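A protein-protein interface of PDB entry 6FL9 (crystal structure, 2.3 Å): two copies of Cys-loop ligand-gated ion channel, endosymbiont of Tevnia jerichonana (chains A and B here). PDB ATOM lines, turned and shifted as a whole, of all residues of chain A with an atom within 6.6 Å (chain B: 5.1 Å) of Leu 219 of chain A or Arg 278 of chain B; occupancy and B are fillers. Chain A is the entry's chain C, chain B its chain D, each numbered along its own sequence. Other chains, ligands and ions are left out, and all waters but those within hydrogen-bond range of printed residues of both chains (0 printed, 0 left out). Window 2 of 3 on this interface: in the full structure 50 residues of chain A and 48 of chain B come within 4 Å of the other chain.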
ATOM      1  N   PHE A 215     -35.814  27.317  10.619  1.00  0.00           N
ATOM      2  CA  PHE A 215     -34.578  28.101  10.750  1.00  0.00           C
ATOM      3  C   PHE A 215     -33.478  27.525   9.878  1.00  0.00           C
ATOM      4  O   PHE A 215     -32.727  28.268   9.243  1.00  0.00           O
ATOM      5  CB  PHE A 215     -34.086  28.155  12.213  1.00  0.00           C
ATOM      6  CG  PHE A 215     -34.914  28.945  13.201  1.00  0.00           C
ATOM      7  CD1 PHE A 215     -35.969  29.750  12.772  1.00  0.00           C
ATOM      8  CD2 PHE A 215     -34.656  28.865  14.566  1.00  0.00           C
ATOM      9  CE1 PHE A 215     -36.759  30.440  13.694  1.00  0.00           C
ATOM     10  CE2 PHE A 215     -35.448  29.559  15.481  1.00  0.00           C
ATOM     11  CZ  PHE A 215     -36.474  30.355  15.034  1.00  0.00           C
ATOM     12  N   THR A 216     -33.410  26.200   9.803  1.00  0.00           N
ATOM     13  CA  THR A 216     -32.384  25.509   9.039  1.00  0.00           C
ATOM     14  C   THR A 216     -32.552  25.674   7.528  1.00  0.00           C
ATOM     15  O   THR A 216     -31.604  25.378   6.797  1.00  0.00           O
ATOM     16  CB  THR A 216     -32.274  24.065   9.455  1.00  0.00           C
ATOM     17  OG1 THR A 216     -33.446  23.399   9.004  1.00  0.00           O
ATOM     18  CG2 THR A 216     -32.067  23.908  10.957  1.00  0.00           C
ATOM     19  N   PHE A 217     -33.698  26.215   7.049  1.00  0.00           N
ATOM     20  CA  PHE A 217     -33.847  26.474   5.612  1.00  0.00           C
ATOM     21  C   PHE A 217     -32.826  27.510   5.144  1.00  0.00           C
ATOM     22  O   PHE A 217     -32.334  27.403   4.031  1.00  0.00           O
ATOM     23  CB  PHE A 217     -35.266  26.889   5.257  1.00  0.00           C
ATOM     24  CG  PHE A 217     -36.196  25.709   5.091  1.00  0.00           C
ATOM     25  CD1 PHE A 217     -36.298  24.729   6.086  1.00  0.00           C
ATOM     26  CD2 PHE A 217     -37.014  25.600   3.968  1.00  0.00           C
ATOM     27  CE1 PHE A 217     -37.175  23.649   5.942  1.00  0.00           C
ATOM     28  CE2 PHE A 217     -37.898  24.514   3.826  1.00  0.00           C
ATOM     29  CZ  PHE A 217     -37.974  23.548   4.817  1.00  0.00           C
ATOM     30  N   PHE A 218     -32.415  28.427   6.049  1.00  0.00           N
ATOM     31  CA  PHE A 218     -31.438  29.469   5.794  1.00  0.00           C
ATOM     32  C   PHE A 218     -29.986  28.920   5.610  1.00  0.00           C
ATOM     33  O   PHE A 218     -29.111  29.658   5.174  1.00  0.00           O
ATOM     34  CB  PHE A 218     -31.546  30.562   6.864  1.00  0.00           C
ATOM     35  CG  PHE A 218     -32.890  31.244   6.775  1.00  0.00           C
ATOM     36  CD1 PHE A 218     -33.116  32.250   5.849  1.00  0.00           C
ATOM     37  CD2 PHE A 218     -33.957  30.831   7.577  1.00  0.00           C
ATOM     38  CE1 PHE A 218     -34.382  32.834   5.725  1.00  0.00           C
ATOM     39  CE2 PHE A 218     -35.218  31.413   7.448  1.00  0.00           C
ATOM     40  CZ  PHE A 218     -35.421  32.409   6.520  1.00  0.00           C
ATOM     41  N   LEU A 219     -29.761  27.622   5.850  1.00  0.00           N
ATOM     42  CA  LEU A 219     -28.475  26.973   5.599  1.00  0.00           C
ATOM     43  C   LEU A 219     -28.355  26.627   4.093  1.00  0.00           C
ATOM     44  O   LEU A 219     -27.240  26.321   3.619  1.00  0.00           O
ATOM     45  CB  LEU A 219     -28.346  25.659   6.391  1.00  0.00           C
ATOM     46  CG  LEU A 219     -28.282  25.732   7.895  1.00  0.00           C
ATOM     47  CD1 LEU A 219     -28.249  24.326   8.468  1.00  0.00           C
ATOM     48  CD2 LEU A 219     -27.102  26.599   8.395  1.00  0.00           C
ATOM     49  N   GLN A 220     -29.505  26.624   3.354  1.00  0.00           N
ATOM     50  CA  GLN A 220     -29.589  26.323   1.917  1.00  0.00           C
ATOM     51  C   GLN A 220     -28.983  24.931   1.557  1.00  0.00           C
ATOM     52  O   GLN A 220     -28.377  24.778   0.485  1.00  0.00           O
ATOM     53  CB  GLN A 220     -28.960  27.452   1.063  1.00  0.00           C
ATOM     54  CG  GLN A 220     -29.472  28.849   1.377  1.00  0.00           C
ATOM     55  CD  GLN A 220     -28.399  29.934   1.321  1.00  0.00           C
ATOM     56  OE1 GLN A 220     -27.379  29.919   2.057  1.00  0.00           O
ATOM     57  NE2 GLN A 220     -28.640  30.940   0.488  1.00  0.00           N
ATOM     58  N   ASP A 221     -29.149  23.928   2.466  1.00  0.00           N
ATOM     59  CA  ASP A 221     -28.688  22.554   2.261  1.00  0.00           C
ATOM     60  C   ASP A 221     -29.939  21.699   2.121  1.00  0.00           C
ATOM     61  O   ASP A 221     -30.570  21.346   3.134  1.00  0.00           O
ATOM     62  CB  ASP A 221     -27.784  22.081   3.426  1.00  0.00           C
ATOM     63  CG  ASP A 221     -27.169  20.709   3.243  1.00  0.00           C
ATOM     64  OD1 ASP A 221     -27.840  19.819   2.648  1.00  0.00           O
ATOM     65  OD2 ASP A 221     -26.061  20.487   3.758  1.00  0.00           O
ATOM     66  N   TYR A 222     -30.310  21.385   0.861  1.00  0.00           N
ATOM     67  CA  TYR A 222     -31.518  20.610   0.526  1.00  0.00           C
ATOM     68  C   TYR A 222     -31.535  19.219   1.126  1.00  0.00           C
ATOM     69  O   TYR A 222     -32.591  18.810   1.632  1.00  0.00           O
ATOM     70  CB  TYR A 222     -31.810  20.568  -0.977  1.00  0.00           C
ATOM     71  CG  TYR A 222     -31.734  21.933  -1.627  1.00  0.00           C
ATOM     72  CD1 TYR A 222     -32.449  23.017  -1.110  1.00  0.00           C
ATOM     73  CD2 TYR A 222     -30.934  22.150  -2.757  1.00  0.00           C
ATOM     74  CE1 TYR A 222     -32.357  24.288  -1.683  1.00  0.00           C
ATOM     75  CE2 TYR A 222     -30.857  23.416  -3.355  1.00  0.00           C
ATOM     76  CZ  TYR A 222     -31.553  24.488  -2.800  1.00  0.00           C
ATOM     77  OH  TYR A 222     -31.455  25.745  -3.363  1.00  0.00           O
ATOM     78  N   LYS A 224     -30.053  18.264   3.959  1.00  0.00           N
ATOM     79  CA  LYS A 224     -30.283  18.486   5.377  1.00  0.00           C
ATOM     80  C   LYS A 224     -31.770  18.760   5.669  1.00  0.00           C
ATOM     81  O   LYS A 224     -32.282  18.250   6.670  1.00  0.00           O
ATOM     82  CB  LYS A 224     -29.353  19.589   5.905  1.00  0.00           C
ATOM     83  CG  LYS A 224     -29.351  19.712   7.426  1.00  0.00           C
ATOM     84  CD  LYS A 224     -28.123  20.437   7.964  1.00  0.00           C
ATOM     85  CE  LYS A 224     -28.272  20.674   9.451  1.00  0.00           C
ATOM     86  NZ  LYS A 224     -27.131  21.419  10.051  1.00  0.00           N
ATOM     87  N   ARG A 225     -32.478  19.489   4.769  1.00  0.00           N
ATOM     88  CA  ARG A 225     -33.927  19.705   4.961  1.00  0.00           C
ATOM     89  C   ARG A 225     -34.657  18.361   4.817  1.00  0.00           C
ATOM     90  O   ARG A 225     -35.493  18.052   5.653  1.00  0.00           O
ATOM     91  CB  ARG A 225     -34.505  20.707   3.971  1.00  0.00           C
ATOM     92  CG  ARG A 225     -33.868  22.089   4.047  1.00  0.00           C
ATOM     93  CD  ARG A 225     -34.234  22.857   2.814  1.00  0.00           C
ATOM     94  NE  ARG A 225     -33.685  24.196   2.760  1.00  0.00           N
ATOM     95  CZ  ARG A 225     -34.000  25.085   1.820  1.00  0.00           C
ATOM     96  NH1 ARG A 225     -34.868  24.771   0.865  1.00  0.00           N
ATOM     97  NH2 ARG A 225     -33.465  26.293   1.833  1.00  0.00           N
ATOM     98  N   ARG A 290     -31.537  27.614  -6.487  1.00  0.00           N
ATOM     99  CA  ARG A 290     -31.336  28.750  -5.578  1.00  0.00           C
ATOM    100  C   ARG A 290     -32.368  29.870  -5.789  1.00  0.00           C
ATOM    101  O   ARG A 290     -32.778  30.490  -4.814  1.00  0.00           O
ATOM    102  CB  ARG A 290     -29.898  29.282  -5.647  1.00  0.00           C
ATOM    103  CG  ARG A 290     -29.497  29.994  -4.357  1.00  0.00           C
ATOM    104  CD  ARG A 290     -28.115  29.610  -3.858  1.00  0.00           C
ATOM    105  NE  ARG A 290     -28.082  28.270  -3.264  1.00  0.00           N
ATOM    106  CZ  ARG A 290     -26.980  27.669  -2.820  1.00  0.00           C
ATOM    107  NH1 ARG A 290     -27.046  26.447  -2.305  1.00  0.00           N
ATOM    108  NH2 ARG A 290     -25.801  28.280  -2.898  1.00  0.00           N
ATOM    109  N   TYR B 222     -20.306  24.937  13.259  1.00  0.00           N
ATOM    110  CA  TYR B 222     -21.659  25.474  13.383  1.00  0.00           C
ATOM    111  C   TYR B 222     -22.746  24.477  13.024  1.00  0.00           C
ATOM    112  O   TYR B 222     -23.737  24.417  13.748  1.00  0.00           O
ATOM    113  CB  TYR B 222     -21.824  26.796  12.607  1.00  0.00           C
ATOM    114  CG  TYR B 222     -20.729  27.801  12.899  1.00  0.00           C
ATOM    115  CD1 TYR B 222     -20.371  28.117  14.209  1.00  0.00           C
ATOM    116  CD2 TYR B 222     -20.055  28.445  11.867  1.00  0.00           C
ATOM    117  CE1 TYR B 222     -19.335  29.022  14.480  1.00  0.00           C
ATOM    118  CE2 TYR B 222     -19.036  29.364  12.128  1.00  0.00           C
ATOM    119  CZ  TYR B 222     -18.663  29.631  13.435  1.00  0.00           C
ATOM    120  OH  TYR B 222     -17.636  30.515  13.685  1.00  0.00           O
ATOM    121  N   THR B 223     -22.534  23.650  11.982  1.00  0.00           N
ATOM    122  CA  THR B 223     -23.476  22.607  11.562  1.00  0.00           C
ATOM    123  C   THR B 223     -23.682  21.606  12.711  1.00  0.00           C
ATOM    124  O   THR B 223     -24.830  21.299  13.071  1.00  0.00           O
ATOM    125  CB  THR B 223     -23.003  21.968  10.251  1.00  0.00           C
ATOM    126  OG1 THR B 223     -23.130  22.923   9.201  1.00  0.00           O
ATOM    127  CG2 THR B 223     -23.781  20.715   9.879  1.00  0.00           C
ATOM    128  N   ILE B 226     -25.871  22.983  15.395  1.00  0.00           N
ATOM    129  CA  ILE B 226     -27.263  22.961  14.936  1.00  0.00           C
ATOM    130  C   ILE B 226     -27.861  21.548  15.140  1.00  0.00           C
ATOM    131  O   ILE B 226     -28.924  21.412  15.747  1.00  0.00           O
ATOM    132  CB  ILE B 226     -27.432  23.512  13.492  1.00  0.00           C
ATOM    133  CG1 ILE B 226     -26.966  24.980  13.398  1.00  0.00           C
ATOM    134  CG2 ILE B 226     -28.893  23.402  13.047  1.00  0.00           C
ATOM    135  CD1 ILE B 226     -26.477  25.419  11.993  1.00  0.00           C
ATOM    136  N   ASN B 274     -26.530  29.762  15.401  1.00  0.00           N
ATOM    137  CA  ASN B 274     -25.584  28.936  14.685  1.00  0.00           C
ATOM    138  C   ASN B 274     -25.982  28.743  13.245  1.00  0.00           C
ATOM    139  O   ASN B 274     -25.084  28.515  12.424  1.00  0.00           O
ATOM    140  CB  ASN B 274     -25.309  27.628  15.420  1.00  0.00           C
ATOM    141  CG  ASN B 274     -24.493  27.935  16.652  1.00  0.00           C
ATOM    142  OD1 ASN B 274     -23.290  28.209  16.571  1.00  0.00           O
ATOM    143  ND2 ASN B 274     -25.172  28.163  17.771  1.00  0.00           N
ATOM    144  N   VAL B 275     -27.289  28.928  12.907  1.00  0.00           N
ATOM    145  CA  VAL B 275     -27.712  28.909  11.506  1.00  0.00           C
ATOM    146  C   VAL B 275     -27.105  30.155  10.851  1.00  0.00           C
ATOM    147  O   VAL B 275     -26.458  30.061   9.791  1.00  0.00           O
ATOM    148  CB  VAL B 275     -29.244  28.823  11.310  1.00  0.00           C
ATOM    149  CG1 VAL B 275     -29.680  29.421   9.965  1.00  0.00           C
ATOM    150  CG2 VAL B 275     -29.731  27.386  11.450  1.00  0.00           C
ATOM    151  N   TRP B 276     -27.220  31.293  11.551  1.00  0.00           N
ATOM    152  CA  TRP B 276     -26.710  32.573  11.079  1.00  0.00           C
ATOM    153  C   TRP B 276     -25.153  32.538  10.847  1.00  0.00           C
ATOM    154  O   TRP B 276     -24.714  32.854   9.736  1.00  0.00           O
ATOM    155  CB  TRP B 276     -27.186  33.733  11.959  1.00  0.00           C
ATOM    156  CG  TRP B 276     -26.935  35.045  11.301  1.00  0.00           C
ATOM    157  CD1 TRP B 276     -27.370  35.441  10.068  1.00  0.00           C
ATOM    158  CD2 TRP B 276     -26.038  36.067  11.757  1.00  0.00           C
ATOM    159  NE1 TRP B 276     -26.853  36.673   9.758  1.00  0.00           N
ATOM    160  CE2 TRP B 276     -26.029  37.084  10.776  1.00  0.00           C
ATOM    161  CE3 TRP B 276     -25.279  36.244  12.930  1.00  0.00           C
ATOM    162  CZ2 TRP B 276     -25.248  38.253  10.907  1.00  0.00           C
ATOM    163  CZ3 TRP B 276     -24.549  37.415  13.083  1.00  0.00           C
ATOM    164  CH2 TRP B 276     -24.505  38.391  12.064  1.00  0.00           C
ATOM    165  N   LEU B 277     -24.362  32.046  11.836  1.00  0.00           N
ATOM    166  CA  LEU B 277     -22.900  31.907  11.732  1.00  0.00           C
ATOM    167  C   LEU B 277     -22.487  31.020  10.547  1.00  0.00           C
ATOM    168  O   LEU B 277     -21.548  31.344   9.832  1.00  0.00           O
ATOM    169  CB  LEU B 277     -22.279  31.363  13.035  1.00  0.00           C
ATOM    170  CG  LEU B 277     -22.345  32.264  14.263  1.00  0.00           C
ATOM    171  CD1 LEU B 277     -21.840  31.544  15.494  1.00  0.00           C
ATOM    172  CD2 LEU B 277     -21.539  33.545  14.066  1.00  0.00           C
ATOM    173  N   ARG B 278     -23.212  29.920  10.319  1.00  0.00           N
ATOM    174  CA  ARG B 278     -22.949  29.024   9.199  1.00  0.00           C
ATOM    175  C   ARG B 278     -23.402  29.655   7.888  1.00  0.00           C
ATOM    176  O   ARG B 278     -22.808  29.358   6.854  1.00  0.00           O
ATOM    177  CB  ARG B 278     -23.590  27.646   9.442  1.00  0.00           C
ATOM    178  CG  ARG B 278     -23.390  26.645   8.303  1.00  0.00           C
ATOM    179  CD  ARG B 278     -21.939  26.245   8.115  1.00  0.00           C
ATOM    180  NE  ARG B 278     -21.808  25.284   7.032  1.00  0.00           N
ATOM    181  CZ  ARG B 278     -20.663  24.995   6.435  1.00  0.00           C
ATOM    182  NH1 ARG B 278     -19.542  25.599   6.806  1.00  0.00           N
ATOM    183  NH2 ARG B 278     -20.628  24.110   5.451  1.00  0.00           N
ATOM    184  N   ARG B 279     -24.417  30.554   7.924  1.00  0.00           N
ATOM    185  CA  ARG B 279     -24.835  31.263   6.712  1.00  0.00           C
ATOM    186  C   ARG B 279     -23.707  32.240   6.330  1.00  0.00           C
ATOM    187  O   ARG B 279     -23.423  32.410   5.139  1.00  0.00           O
ATOM    188  CB  ARG B 279     -26.191  31.987   6.874  1.00  0.00           C
ATOM    189  CG  ARG B 279     -26.761  32.432   5.515  1.00  0.00           C
ATOM    190  CD  ARG B 279     -28.139  33.048   5.598  1.00  0.00           C
ATOM    191  NE  ARG B 279     -28.529  33.639   4.312  1.00  0.00           N
ATOM    192  CZ  ARG B 279     -29.428  33.122   3.474  1.00  0.00           C
ATOM    193  NH1 ARG B 279     -30.100  32.016   3.800  1.00  0.00           N
ATOM    194  NH2 ARG B 279     -29.698  33.733   2.324  1.00  0.00           N
ATOM    195  N   LEU B 280     -23.025  32.834   7.343  1.00  0.00           N
ATOM    196  CA  LEU B 280     -21.889  33.735   7.112  1.00  0.00           C
ATOM    197  C   LEU B 280     -20.745  32.964   6.424  1.00  0.00           C
ATOM    198  O   LEU B 280     -20.221  33.434   5.406  1.00  0.00           O
ATOM    199  CB  LEU B 280     -21.411  34.404   8.422  1.00  0.00           C
ATOM    200  CG  LEU B 280     -22.348  35.450   9.053  1.00  0.00           C
ATOM    201  CD1 LEU B 280     -21.815  35.905  10.385  1.00  0.00           C
ATOM    202  CD2 LEU B 280     -22.518  36.675   8.144  1.00  0.00           C
ATOM    203  N   GLU B 281     -20.403  31.759   6.936  1.00  0.00           N
ATOM    204  CA  GLU B 281     -19.352  30.906   6.370  1.00  0.00           C
ATOM    205  C   GLU B 281     -19.677  30.553   4.921  1.00  0.00           C
ATOM    206  O   GLU B 281     -18.781  30.497   4.107  1.00  0.00           O
ATOM    207  CB  GLU B 281     -19.231  29.598   7.161  1.00  0.00           C
ATOM    208  CG  GLU B 281     -18.347  29.629   8.394  1.00  0.00           C
ATOM    209  CD  GLU B 281     -17.973  28.238   8.888  1.00  0.00           C
ATOM    210  OE1 GLU B 281     -18.873  27.365   8.958  1.00  0.00           O
ATOM    211  OE2 GLU B 281     -16.784  28.016   9.212  1.00  0.00           O
ATOM    212  N   ASN B 282     -20.957  30.303   4.605  1.00  0.00           N
ATOM    213  CA  ASN B 282     -21.410  29.924   3.261  1.00  0.00           C
ATOM    214  C   ASN B 282     -21.337  31.063   2.294  1.00  0.00           C
ATOM    215  O   ASN B 282     -21.282  30.820   1.089  1.00  0.00           O
ATOM    216  CB  ASN B 282     -22.843  29.359   3.296  1.00  0.00           C
ATOM    217  CG  ASN B 282     -22.949  28.030   3.960  1.00  0.00           C
ATOM    218  OD1 ASN B 282     -21.973  27.265   4.020  1.00  0.00           O
ATOM    219  ND2 ASN B 282     -24.155  27.729   4.462  1.00  0.00           N
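The backbone carbonyl oxygen of Phe 218 of chain A lies within hydrogen-bond range of the guanidinium group of Arg 279 of chain B, at 2.9 Å. The side-chain amide nitrogen (ND2) of Asn 282 of chain B is in hydrogen-bond range of the backbone carbonyl oxygen (O) of Leu 219 of chain A, 3.5 Å away.
Val 275 of chain B touches Phe 215 of chain A (CG1 to O, 3.3 Å). Ile 226 of chain B touches Thr 216 of chain A. Phe 218 of chain A touches Val 275 of chain B. Leu 219 of chain A touches Ile 226 of chain B (CD2 to CD1, 3.8 Å). Leu 219 of chain A touches Val 275 of chain B (CD2 to O, 3.8 Å). Arg 278 of chain B touches Leu 219 of chain A (CG to CD2, 3.7 Å). Gln 220 of chain A touches Arg 279 of chain B. Thr 223 of chain B touches Lys 224 of chain A (CG2 to NZ, 3.4 Å).
The backbone NH of Lys 224 of chain A sits at hydrogen-bond distance from the side-chain carboxylate of Asp 221 of chain A (3.0 Å). OG1 of Thr 223 of chain B sits at hydrogen-bond distance from NE of Arg 278 of chain B (3.5 Å). OE1 of Glu 281 of chain B lies within salt-bridge range of NH1 of Arg 278 of chain B. The backbone carbonyl oxygen (O) of Arg 278 of chain B lies close to the side-chain amide nitrogen (ND2) of Asn 282 of chain B, at 3.2 Å.
Of the printed residues of chain A, Arg 278 of chain B touches Leu 219 (3.7 Å). Printed residues of chain A within 4 Å of Asn 282 of chain B: Leu 219 (3.5 Å). Printed residues of chain A within 4 Å of Arg 279 of chain B: Phe 218 and Gln 220. Tyr 222 of chain A touches none of the printed residues of chain B. The nearest residue of chain A that does not touch Arg 278 of chain B is Phe 218 of chain A (6.3 Å). The nearest printed residue of chain B that does not touch Phe 215 of chain A is Trp 276 of chain B (6.7 Å).
Position printed for both chains: 222.
Hydrophobic or aromatic side chains of chain A within 4 Å of the printed part of chain B: Phe 218 and Leu 219. Hydrophobic or aromatic side chains of chain B that line the printed part of chain A: Ile 226 and Val 275. Along chain B the printed residues that touch a printed residue of chain A span positions 223 to 282. Among the printed residues, no Asp or Glu carboxylate lies within 4 Å of a Lys or Arg side-chain nitrogen of the other chain.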
